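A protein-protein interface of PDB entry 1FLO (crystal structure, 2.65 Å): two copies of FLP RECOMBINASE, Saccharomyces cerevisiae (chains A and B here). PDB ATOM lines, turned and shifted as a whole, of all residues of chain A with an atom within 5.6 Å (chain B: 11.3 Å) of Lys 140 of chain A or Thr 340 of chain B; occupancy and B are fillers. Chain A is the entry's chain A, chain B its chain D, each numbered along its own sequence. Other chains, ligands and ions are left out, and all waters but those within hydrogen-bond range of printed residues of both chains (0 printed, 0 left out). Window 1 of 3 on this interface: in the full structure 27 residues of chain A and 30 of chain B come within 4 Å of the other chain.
The side-chain hydroxyl (OG1) of Thr 340 of chain B lies close to the backbone carbonyl oxygen (O) of Ala 336 of chain B (3.4 Å). NE2 of His 344 of chain B sits close to O of Thr 341 of chain B, 3.4 Å away. A ring nitrogen (NE2) of His 344 of chain B lies close to the backbone carbonyl oxygen of Tyr 342 of chain B (3.4 Å).
Hydrophobic or aromatic side chains of chain B within 4 Å of the printed part of chain A: His 344. Of the 10 printed residues of chain A, 3 touch a printed residue of chain B. Printed residues of chain A that touch a printed residue of chain B: Lys 140, Leu 143 and Lys 144. Hydrophobic or aromatic side chains of chain A within 4 Å of the printed part of chain B: Leu 143. Among the printed residues, 3 pairs touch across the chains. Among the printed residues, no Asp or Glu carboxylate lies within 4 Å of a Lys or Arg side-chain nitrogen of the other chain.
Among the printed residues, merely in contact across the chains: Lys 140 of chain A with Thr 340 of chain B (3.8 Å) and Leu 143 of chain A with His 344 of chain B (3.7 Å).
NZ of Lys 144 of chain A sits at hydrogen-bond distance from ND1 of His 344 of chain B, at 3.1 Å.
Of the printed residues of chain B, Lys 140 of chain A touches Thr 340 (3.8 Å). Of chain A, only Lys 140 (3.8 Å) comes within 4 Å of Thr 340 of chain B. No residue of chain B comes within 4 Å of Asn 136 of chain A. No residue of chain B comes within 4 Å of Ser 137 of chain A. No residue of chain B comes within 4 Å of Ser 139 of chain A. Leu 143 of chain A touches just one residue of chain B: His 344. Of the printed residues of chain A, His 344 of chain B touches Leu 143 and Lys 144. Printed residues of chain B within 4 Å of Lys 144 of chain A: His 344 (3.1 Å). The nearest printed residue of chain A that does not touch His 344 of chain B is Lys 140 of chain A (4.9 Å).
No position is printed for both chains. Of the 3 pairs that touch across the chains among the printed residues, none has its exchanged pair printed and touching as well.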
ATOM      1  N   ASN A 136      14.333  14.618   0.649  1.00  0.00           N
ATOM      2  CA  ASN A 136      13.506  14.786   1.839  1.00  0.00           C
ATOM      3  C   ASN A 136      12.205  15.475   1.439  1.00  0.00           C
ATOM      4  O   ASN A 136      11.120  15.080   1.870  1.00  0.00           O
ATOM      5  CB  ASN A 136      14.231  15.645   2.879  1.00  0.00           C
ATOM      6  CG  ASN A 136      15.268  14.866   3.659  1.00  0.00           C
ATOM      7  OD1 ASN A 136      15.965  15.422   4.511  1.00  0.00           O
ATOM      8  ND2 ASN A 136      15.370  13.568   3.379  1.00  0.00           N
ATOM      9  N   SER A 137      12.327  16.509   0.610  1.00  0.00           N
ATOM     10  CA  SER A 137      11.167  17.255   0.144  1.00  0.00           C
ATOM     11  C   SER A 137      10.169  16.328  -0.538  1.00  0.00           C
ATOM     12  O   SER A 137       8.971  16.376  -0.254  1.00  0.00           O
ATOM     13  CB  SER A 137      11.594  18.351  -0.837  1.00  0.00           C
ATOM     14  OG  SER A 137      12.538  19.230  -0.251  1.00  0.00           O
ATOM     15  N   HIS A 138      10.661  15.481  -1.437  1.00  0.00           N
ATOM     16  CA  HIS A 138       9.777  14.565  -2.148  1.00  0.00           C
ATOM     17  C   HIS A 138       9.145  13.583  -1.175  1.00  0.00           C
ATOM     18  O   HIS A 138       8.019  13.121  -1.370  1.00  0.00           O
ATOM     19  CB  HIS A 138      10.550  13.793  -3.218  1.00  0.00           C
ATOM     20  CG  HIS A 138       9.673  12.971  -4.110  1.00  0.00           C
ATOM     21  ND1 HIS A 138       8.723  13.530  -4.939  1.00  0.00           N
ATOM     22  CD2 HIS A 138       9.576  11.630  -4.277  1.00  0.00           C
ATOM     23  CE1 HIS A 138       8.078  12.569  -5.576  1.00  0.00           C
ATOM     24  NE2 HIS A 138       8.576  11.407  -5.191  1.00  0.00           N
ATOM     25  N   SER A 139       9.884  13.285  -0.118  1.00  0.00           N
ATOM     26  CA  SER A 139       9.445  12.355   0.905  1.00  0.00           C
ATOM     27  C   SER A 139       8.316  12.920   1.765  1.00  0.00           C
ATOM     28  O   SER A 139       7.369  12.216   2.097  1.00  0.00           O
ATOM     29  CB  SER A 139      10.641  11.978   1.769  1.00  0.00           C
ATOM     30  OG  SER A 139      10.282  11.048   2.763  1.00  0.00           O
ATOM     31  N   LYS A 140       8.421  14.189   2.137  1.00  0.00           N
ATOM     32  CA  LYS A 140       7.389  14.818   2.951  1.00  0.00           C
ATOM     33  C   LYS A 140       6.150  14.974   2.101  1.00  0.00           C
ATOM     34  O   LYS A 140       5.050  14.649   2.530  1.00  0.00           O
ATOM     35  CB  LYS A 140       7.848  16.189   3.448  1.00  0.00           C
ATOM     36  CG  LYS A 140       9.002  16.117   4.424  1.00  0.00           C
ATOM     37  CD  LYS A 140       9.444  17.475   4.941  1.00  0.00           C
ATOM     38  CE  LYS A 140      10.605  17.300   5.910  1.00  0.00           C
ATOM     39  NZ  LYS A 140      11.129  18.586   6.436  1.00  0.00           N
ATOM     40  N   LYS A 141       6.339  15.472   0.886  1.00  0.00           N
ATOM     41  CA  LYS A 141       5.232  15.657  -0.032  1.00  0.00           C
ATOM     42  C   LYS A 141       4.344  14.422   0.016  1.00  0.00           C
ATOM     43  O   LYS A 141       3.151  14.511   0.350  1.00  0.00           O
ATOM     44  CB  LYS A 141       5.755  15.850  -1.454  1.00  0.00           C
ATOM     45  CG  LYS A 141       4.669  16.108  -2.494  1.00  0.00           C
ATOM     46  CD  LYS A 141       3.958  17.443  -2.256  1.00  0.00           C
ATOM     47  CE  LYS A 141       2.982  17.766  -3.392  1.00  0.00           C
ATOM     48  NZ  LYS A 141       2.299  19.085  -3.217  1.00  0.00           N
ATOM     49  N   MET A 142       4.931  13.268  -0.296  1.00  0.00           N
ATOM     50  CA  MET A 142       4.163  12.035  -0.299  1.00  0.00           C
ATOM     51  C   MET A 142       3.494  11.761   1.036  1.00  0.00           C
ATOM     52  O   MET A 142       2.324  11.405   1.066  1.00  0.00           O
ATOM     53  CB  MET A 142       5.043  10.861  -0.711  1.00  0.00           C
ATOM     54  CG  MET A 142       5.658  11.036  -2.096  1.00  0.00           C
ATOM     55  SD  MET A 142       4.463  11.522  -3.377  1.00  0.00           S
ATOM     56  CE  MET A 142       3.793   9.944  -3.809  1.00  0.00           C
ATOM     57  N   LEU A 143       4.217  11.944   2.140  1.00  0.00           N
ATOM     58  CA  LEU A 143       3.633  11.703   3.454  1.00  0.00           C
ATOM     59  C   LEU A 143       2.380  12.552   3.685  1.00  0.00           C
ATOM     60  O   LEU A 143       1.378  12.042   4.189  1.00  0.00           O
ATOM     61  CB  LEU A 143       4.657  11.952   4.557  1.00  0.00           C
ATOM     62  CG  LEU A 143       5.636  10.780   4.746  1.00  0.00           C
ATOM     63  CD1 LEU A 143       6.922  11.231   5.453  1.00  0.00           C
ATOM     64  CD2 LEU A 143       4.936   9.667   5.521  1.00  0.00           C
ATOM     65  N   LYS A 144       2.447  13.830   3.304  1.00  0.00           N
ATOM     66  CA  LYS A 144       1.323  14.762   3.440  1.00  0.00           C
ATOM     67  C   LYS A 144       0.095  14.240   2.712  1.00  0.00           C
ATOM     68  O   LYS A 144      -1.002  14.213   3.272  1.00  0.00           O
ATOM     69  CB  LYS A 144       1.686  16.140   2.873  1.00  0.00           C
ATOM     70  CG  LYS A 144       2.331  17.110   3.878  1.00  0.00           C
ATOM     71  CD  LYS A 144       3.680  16.601   4.420  1.00  0.00           C
ATOM     72  CE  LYS A 144       4.255  17.539   5.484  1.00  0.00           C
ATOM     73  NZ  LYS A 144       5.513  17.042   6.117  1.00  0.00           N
ATOM     74  N   ALA A 145       0.291  13.839   1.459  1.00  0.00           N
ATOM     75  CA  ALA A 145      -0.776  13.289   0.633  1.00  0.00           C
ATOM     76  C   ALA A 145      -1.382  12.030   1.260  1.00  0.00           C
ATOM     77  O   ALA A 145      -2.583  11.986   1.544  1.00  0.00           O
ATOM     78  CB  ALA A 145      -0.235  12.967  -0.732  1.00  0.00           C
ATOM     79  N   THR B 223       3.313  31.787   9.737  1.00  0.00           N
ATOM     80  CA  THR B 223       4.086  30.774  10.444  1.00  0.00           C
ATOM     81  C   THR B 223       4.414  29.613   9.526  1.00  0.00           C
ATOM     82  O   THR B 223       5.104  28.685   9.926  1.00  0.00           O
ATOM     83  CB  THR B 223       3.311  30.234  11.658  1.00  0.00           C
ATOM     84  OG1 THR B 223       2.093  29.619  11.223  1.00  0.00           O
ATOM     85  CG2 THR B 223       2.987  31.365  12.618  1.00  0.00           C
ATOM     86  N   SER B 224       3.906  29.684   8.295  1.00  0.00           N
ATOM     87  CA  SER B 224       4.107  28.654   7.275  1.00  0.00           C
ATOM     88  C   SER B 224       3.336  27.362   7.551  1.00  0.00           C
ATOM     89  O   SER B 224       3.465  26.384   6.827  1.00  0.00           O
ATOM     90  CB  SER B 224       5.597  28.347   7.105  1.00  0.00           C
ATOM     91  OG  SER B 224       6.255  29.429   6.481  1.00  0.00           O
ATOM     92  N   VAL B 225       2.535  27.365   8.606  1.00  0.00           N
ATOM     93  CA  VAL B 225       1.736  26.199   8.941  1.00  0.00           C
ATOM     94  C   VAL B 225       0.356  26.423   8.327  1.00  0.00           C
ATOM     95  O   VAL B 225      -0.403  27.284   8.780  1.00  0.00           O
ATOM     96  CB  VAL B 225       1.604  26.036  10.474  1.00  0.00           C
ATOM     97  CG1 VAL B 225       0.864  24.757  10.811  1.00  0.00           C
ATOM     98  CG2 VAL B 225       2.973  26.019  11.096  1.00  0.00           C
ATOM     99  N   SER B 330       0.894  28.451  16.643  1.00  0.00           N
ATOM    100  CA  SER B 330       1.934  27.432  16.557  1.00  0.00           C
ATOM    101  C   SER B 330       1.952  26.549  17.803  1.00  0.00           C
ATOM    102  O   SER B 330       2.036  27.048  18.924  1.00  0.00           O
ATOM    103  CB  SER B 330       3.290  28.102  16.396  1.00  0.00           C
ATOM    104  OG  SER B 330       3.233  29.066  15.367  1.00  0.00           O
ATOM    105  N   ASP B 331       1.872  25.237  17.612  1.00  0.00           N
ATOM    106  CA  ASP B 331       1.893  24.332  18.747  1.00  0.00           C
ATOM    107  C   ASP B 331       3.267  24.291  19.417  1.00  0.00           C
ATOM    108  O   ASP B 331       4.304  24.503  18.776  1.00  0.00           O
ATOM    109  CB  ASP B 331       1.488  22.924  18.334  1.00  0.00           C
ATOM    110  CG  ASP B 331       1.546  21.953  19.494  1.00  0.00           C
ATOM    111  OD1 ASP B 331       2.651  21.499  19.838  1.00  0.00           O
ATOM    112  OD2 ASP B 331       0.485  21.670  20.084  1.00  0.00           O
ATOM    113  N   LYS B 332       3.262  23.992  20.711  1.00  0.00           N
ATOM    114  CA  LYS B 332       4.484  23.971  21.485  1.00  0.00           C
ATOM    115  C   LYS B 332       4.609  22.756  22.376  1.00  0.00           C
ATOM    116  O   LYS B 332       5.695  22.463  22.858  1.00  0.00           O
ATOM    117  CB  LYS B 332       4.557  25.234  22.341  1.00  0.00           C
ATOM    118  CG  LYS B 332       4.817  26.481  21.544  1.00  0.00           C
ATOM    119  CD  LYS B 332       6.241  26.455  20.973  1.00  0.00           C
ATOM    120  CE  LYS B 332       6.552  27.679  20.103  1.00  0.00           C
ATOM    121  NZ  LYS B 332       5.850  27.665  18.782  1.00  0.00           N
ATOM    122  N   ARG B 333       3.503  22.051  22.581  1.00  0.00           N
ATOM    123  CA  ARG B 333       3.496  20.877  23.437  1.00  0.00           C
ATOM    124  C   ARG B 333       4.349  19.738  22.888  1.00  0.00           C
ATOM    125  O   ARG B 333       5.123  19.118  23.620  1.00  0.00           O
ATOM    126  CB  ARG B 333       2.062  20.399  23.657  1.00  0.00           C
ATOM    127  CG  ARG B 333       1.131  21.465  24.218  1.00  0.00           C
ATOM    128  CD  ARG B 333      -0.271  20.908  24.396  1.00  0.00           C
ATOM    129  NE  ARG B 333      -1.289  21.948  24.305  1.00  0.00           N
ATOM    130  CZ  ARG B 333      -2.584  21.712  24.106  1.00  0.00           C
ATOM    131  NH1 ARG B 333      -3.029  20.462  23.982  1.00  0.00           N
ATOM    132  NH2 ARG B 333      -3.436  22.729  24.017  1.00  0.00           N
ATOM    133  N   ALA B 334       4.199  19.454  21.600  1.00  0.00           N
ATOM    134  CA  ALA B 334       4.975  18.396  20.979  1.00  0.00           C
ATOM    135  C   ALA B 334       6.389  18.893  20.698  1.00  0.00           C
ATOM    136  O   ALA B 334       6.597  20.057  20.334  1.00  0.00           O
ATOM    137  CB  ALA B 334       4.317  17.949  19.699  1.00  0.00           C
ATOM    138  N   SER B 335       7.352  17.998  20.886  1.00  0.00           N
ATOM    139  CA  SER B 335       8.763  18.284  20.671  1.00  0.00           C
ATOM    140  C   SER B 335       9.062  18.841  19.286  1.00  0.00           C
ATOM    141  O   SER B 335       8.347  18.562  18.316  1.00  0.00           O
ATOM    142  CB  SER B 335       9.581  17.012  20.883  1.00  0.00           C
ATOM    143  OG  SER B 335      10.973  17.269  20.810  1.00  0.00           O
ATOM    144  N   ALA B 336      10.136  19.621  19.207  1.00  0.00           N
ATOM    145  CA  ALA B 336      10.584  20.245  17.961  1.00  0.00           C
ATOM    146  C   ALA B 336      10.719  19.289  16.765  1.00  0.00           C
ATOM    147  O   ALA B 336      10.151  19.529  15.703  1.00  0.00           O
ATOM    148  CB  ALA B 336      11.907  20.957  18.197  1.00  0.00           C
ATOM    149  N   VAL B 337      11.477  18.211  16.930  1.00  0.00           N
ATOM    150  CA  VAL B 337      11.672  17.264  15.837  1.00  0.00           C
ATOM    151  C   VAL B 337      10.386  16.549  15.467  1.00  0.00           C
ATOM    152  O   VAL B 337      10.139  16.282  14.290  1.00  0.00           O
ATOM    153  CB  VAL B 337      12.774  16.240  16.191  1.00  0.00           C
ATOM    154  CG1 VAL B 337      12.661  15.002  15.319  1.00  0.00           C
ATOM    155  CG2 VAL B 337      14.133  16.871  15.986  1.00  0.00           C
ATOM    156  N   ALA B 338       9.574  16.241  16.475  1.00  0.00           N
ATOM    157  CA  ALA B 338       8.295  15.577  16.254  1.00  0.00           C
ATOM    158  C   ALA B 338       7.416  16.420  15.303  1.00  0.00           C
ATOM    159  O   ALA B 338       6.772  15.894  14.398  1.00  0.00           O
ATOM    160  CB  ALA B 338       7.602  15.366  17.589  1.00  0.00           C
ATOM    161  N   ARG B 339       7.420  17.734  15.505  1.00  0.00           N
ATOM    162  CA  ARG B 339       6.645  18.660  14.676  1.00  0.00           C
ATOM    163  C   ARG B 339       7.252  18.828  13.276  1.00  0.00           C
ATOM    164  O   ARG B 339       6.544  18.993  12.278  1.00  0.00           O
ATOM    165  CB  ARG B 339       6.590  20.035  15.349  1.00  0.00           C
ATOM    166  CG  ARG B 339       5.718  20.123  16.575  1.00  0.00           C
ATOM    167  CD  ARG B 339       5.693  21.547  17.089  1.00  0.00           C
ATOM    168  NE  ARG B 339       6.997  21.961  17.590  1.00  0.00           N
ATOM    169  CZ  ARG B 339       7.371  23.224  17.756  1.00  0.00           C
ATOM    170  NH1 ARG B 339       6.543  24.214  17.457  1.00  0.00           N
ATOM    171  NH2 ARG B 339       8.571  23.494  18.237  1.00  0.00           N
ATOM    172  N   THR B 340       8.576  18.801  13.240  1.00  0.00           N
ATOM    173  CA  THR B 340       9.380  18.967  12.036  1.00  0.00           C
ATOM    174  C   THR B 340       9.449  17.795  11.042  1.00  0.00           C
ATOM    175  O   THR B 340       9.551  18.001   9.827  1.00  0.00           O
ATOM    176  CB  THR B 340      10.817  19.350  12.453  1.00  0.00           C
ATOM    177  OG1 THR B 340      10.896  20.766  12.647  1.00  0.00           O
ATOM    178  CG2 THR B 340      11.829  18.911  11.423  1.00  0.00           C
ATOM    179  N   THR B 341       9.406  16.564  11.532  1.00  0.00           N
ATOM    180  CA  THR B 341       9.509  15.439  10.609  1.00  0.00           C
ATOM    181  C   THR B 341       8.423  14.377  10.703  1.00  0.00           C
ATOM    182  O   THR B 341       8.345  13.517   9.828  1.00  0.00           O
ATOM    183  CB  THR B 341      10.903  14.748  10.732  1.00  0.00           C
ATOM    184  OG1 THR B 341      11.107  14.324  12.081  1.00  0.00           O
ATOM    185  CG2 THR B 341      12.033  15.717  10.366  1.00  0.00           C
ATOM    186  N   TYR B 342       7.578  14.433  11.731  1.00  0.00           N
ATOM    187  CA  TYR B 342       6.521  13.433  11.875  1.00  0.00           C
ATOM    188  C   TYR B 342       5.072  13.906  11.789  1.00  0.00           C
ATOM    189  O   TYR B 342       4.170  13.090  11.673  1.00  0.00           O
ATOM    190  CB  TYR B 342       6.692  12.679  13.179  1.00  0.00           C
ATOM    191  CG  TYR B 342       7.995  11.954  13.310  1.00  0.00           C
ATOM    192  CD1 TYR B 342       9.143  12.605  13.764  1.00  0.00           C
ATOM    193  CD2 TYR B 342       8.066  10.592  13.071  1.00  0.00           C
ATOM    194  CE1 TYR B 342      10.318  11.908  13.990  1.00  0.00           C
ATOM    195  CE2 TYR B 342       9.237   9.881  13.288  1.00  0.00           C
ATOM    196  CZ  TYR B 342      10.361  10.534  13.752  1.00  0.00           C
ATOM    197  OH  TYR B 342      11.500   9.792  14.011  1.00  0.00           O
ATOM    198  N   THR B 343       4.848  15.209  11.862  1.00  0.00           N
ATOM    199  CA  THR B 343       3.501  15.745  11.798  1.00  0.00           C
ATOM    200  C   THR B 343       3.118  15.993  10.348  1.00  0.00           C
ATOM    201  O   THR B 343       3.708  16.845   9.700  1.00  0.00           O
ATOM    202  CB  THR B 343       3.409  17.065  12.546  1.00  0.00           C
ATOM    203  OG1 THR B 343       4.011  16.927  13.836  1.00  0.00           O
ATOM    204  CG2 THR B 343       1.957  17.462  12.704  1.00  0.00           C
ATOM    205  N   HIS B 344       2.123  15.267   9.841  1.00  0.00           N
ATOM    206  CA  HIS B 344       1.707  15.429   8.446  1.00  0.00           C
ATOM    207  C   HIS B 344       0.218  15.772   8.252  1.00  0.00           C
ATOM    208  O   HIS B 344      -0.285  15.723   7.135  1.00  0.00           O
ATOM    209  CB  HIS B 344       2.058  14.158   7.659  1.00  0.00           C
ATOM    210  CG  HIS B 344       3.458  13.679   7.883  1.00  0.00           C
ATOM    211  ND1 HIS B 344       4.562  14.376   7.442  1.00  0.00           N
ATOM    212  CD2 HIS B 344       3.939  12.613   8.569  1.00  0.00           C
ATOM    213  CE1 HIS B 344       5.660  13.766   7.853  1.00  0.00           C
ATOM    214  NE2 HIS B 344       5.311  12.694   8.540  1.00  0.00           N
ATOM    215  N   GLN B 345      -0.465  16.127   9.338  1.00  0.00           N
ATOM    216  CA  GLN B 345      -1.882  16.494   9.308  1.00  0.00           C
ATOM    217  C   GLN B 345      -2.135  17.603  10.346  1.00  0.00           C
ATOM    218  O   GLN B 345      -1.752  17.475  11.516  1.00  0.00           O
ATOM    219  CB  GLN B 345      -2.727  15.268   9.634  1.00  0.00           C
ATOM    220  CG  GLN B 345      -4.196  15.395   9.323  1.00  0.00           C
ATOM    221  CD  GLN B 345      -4.964  14.124   9.669  1.00  0.00           C
ATOM    222  OE1 GLN B 345      -6.158  14.004   9.386  1.00  0.00           O
ATOM    223  NE2 GLN B 345      -4.277  13.169  10.289  1.00  0.00           N
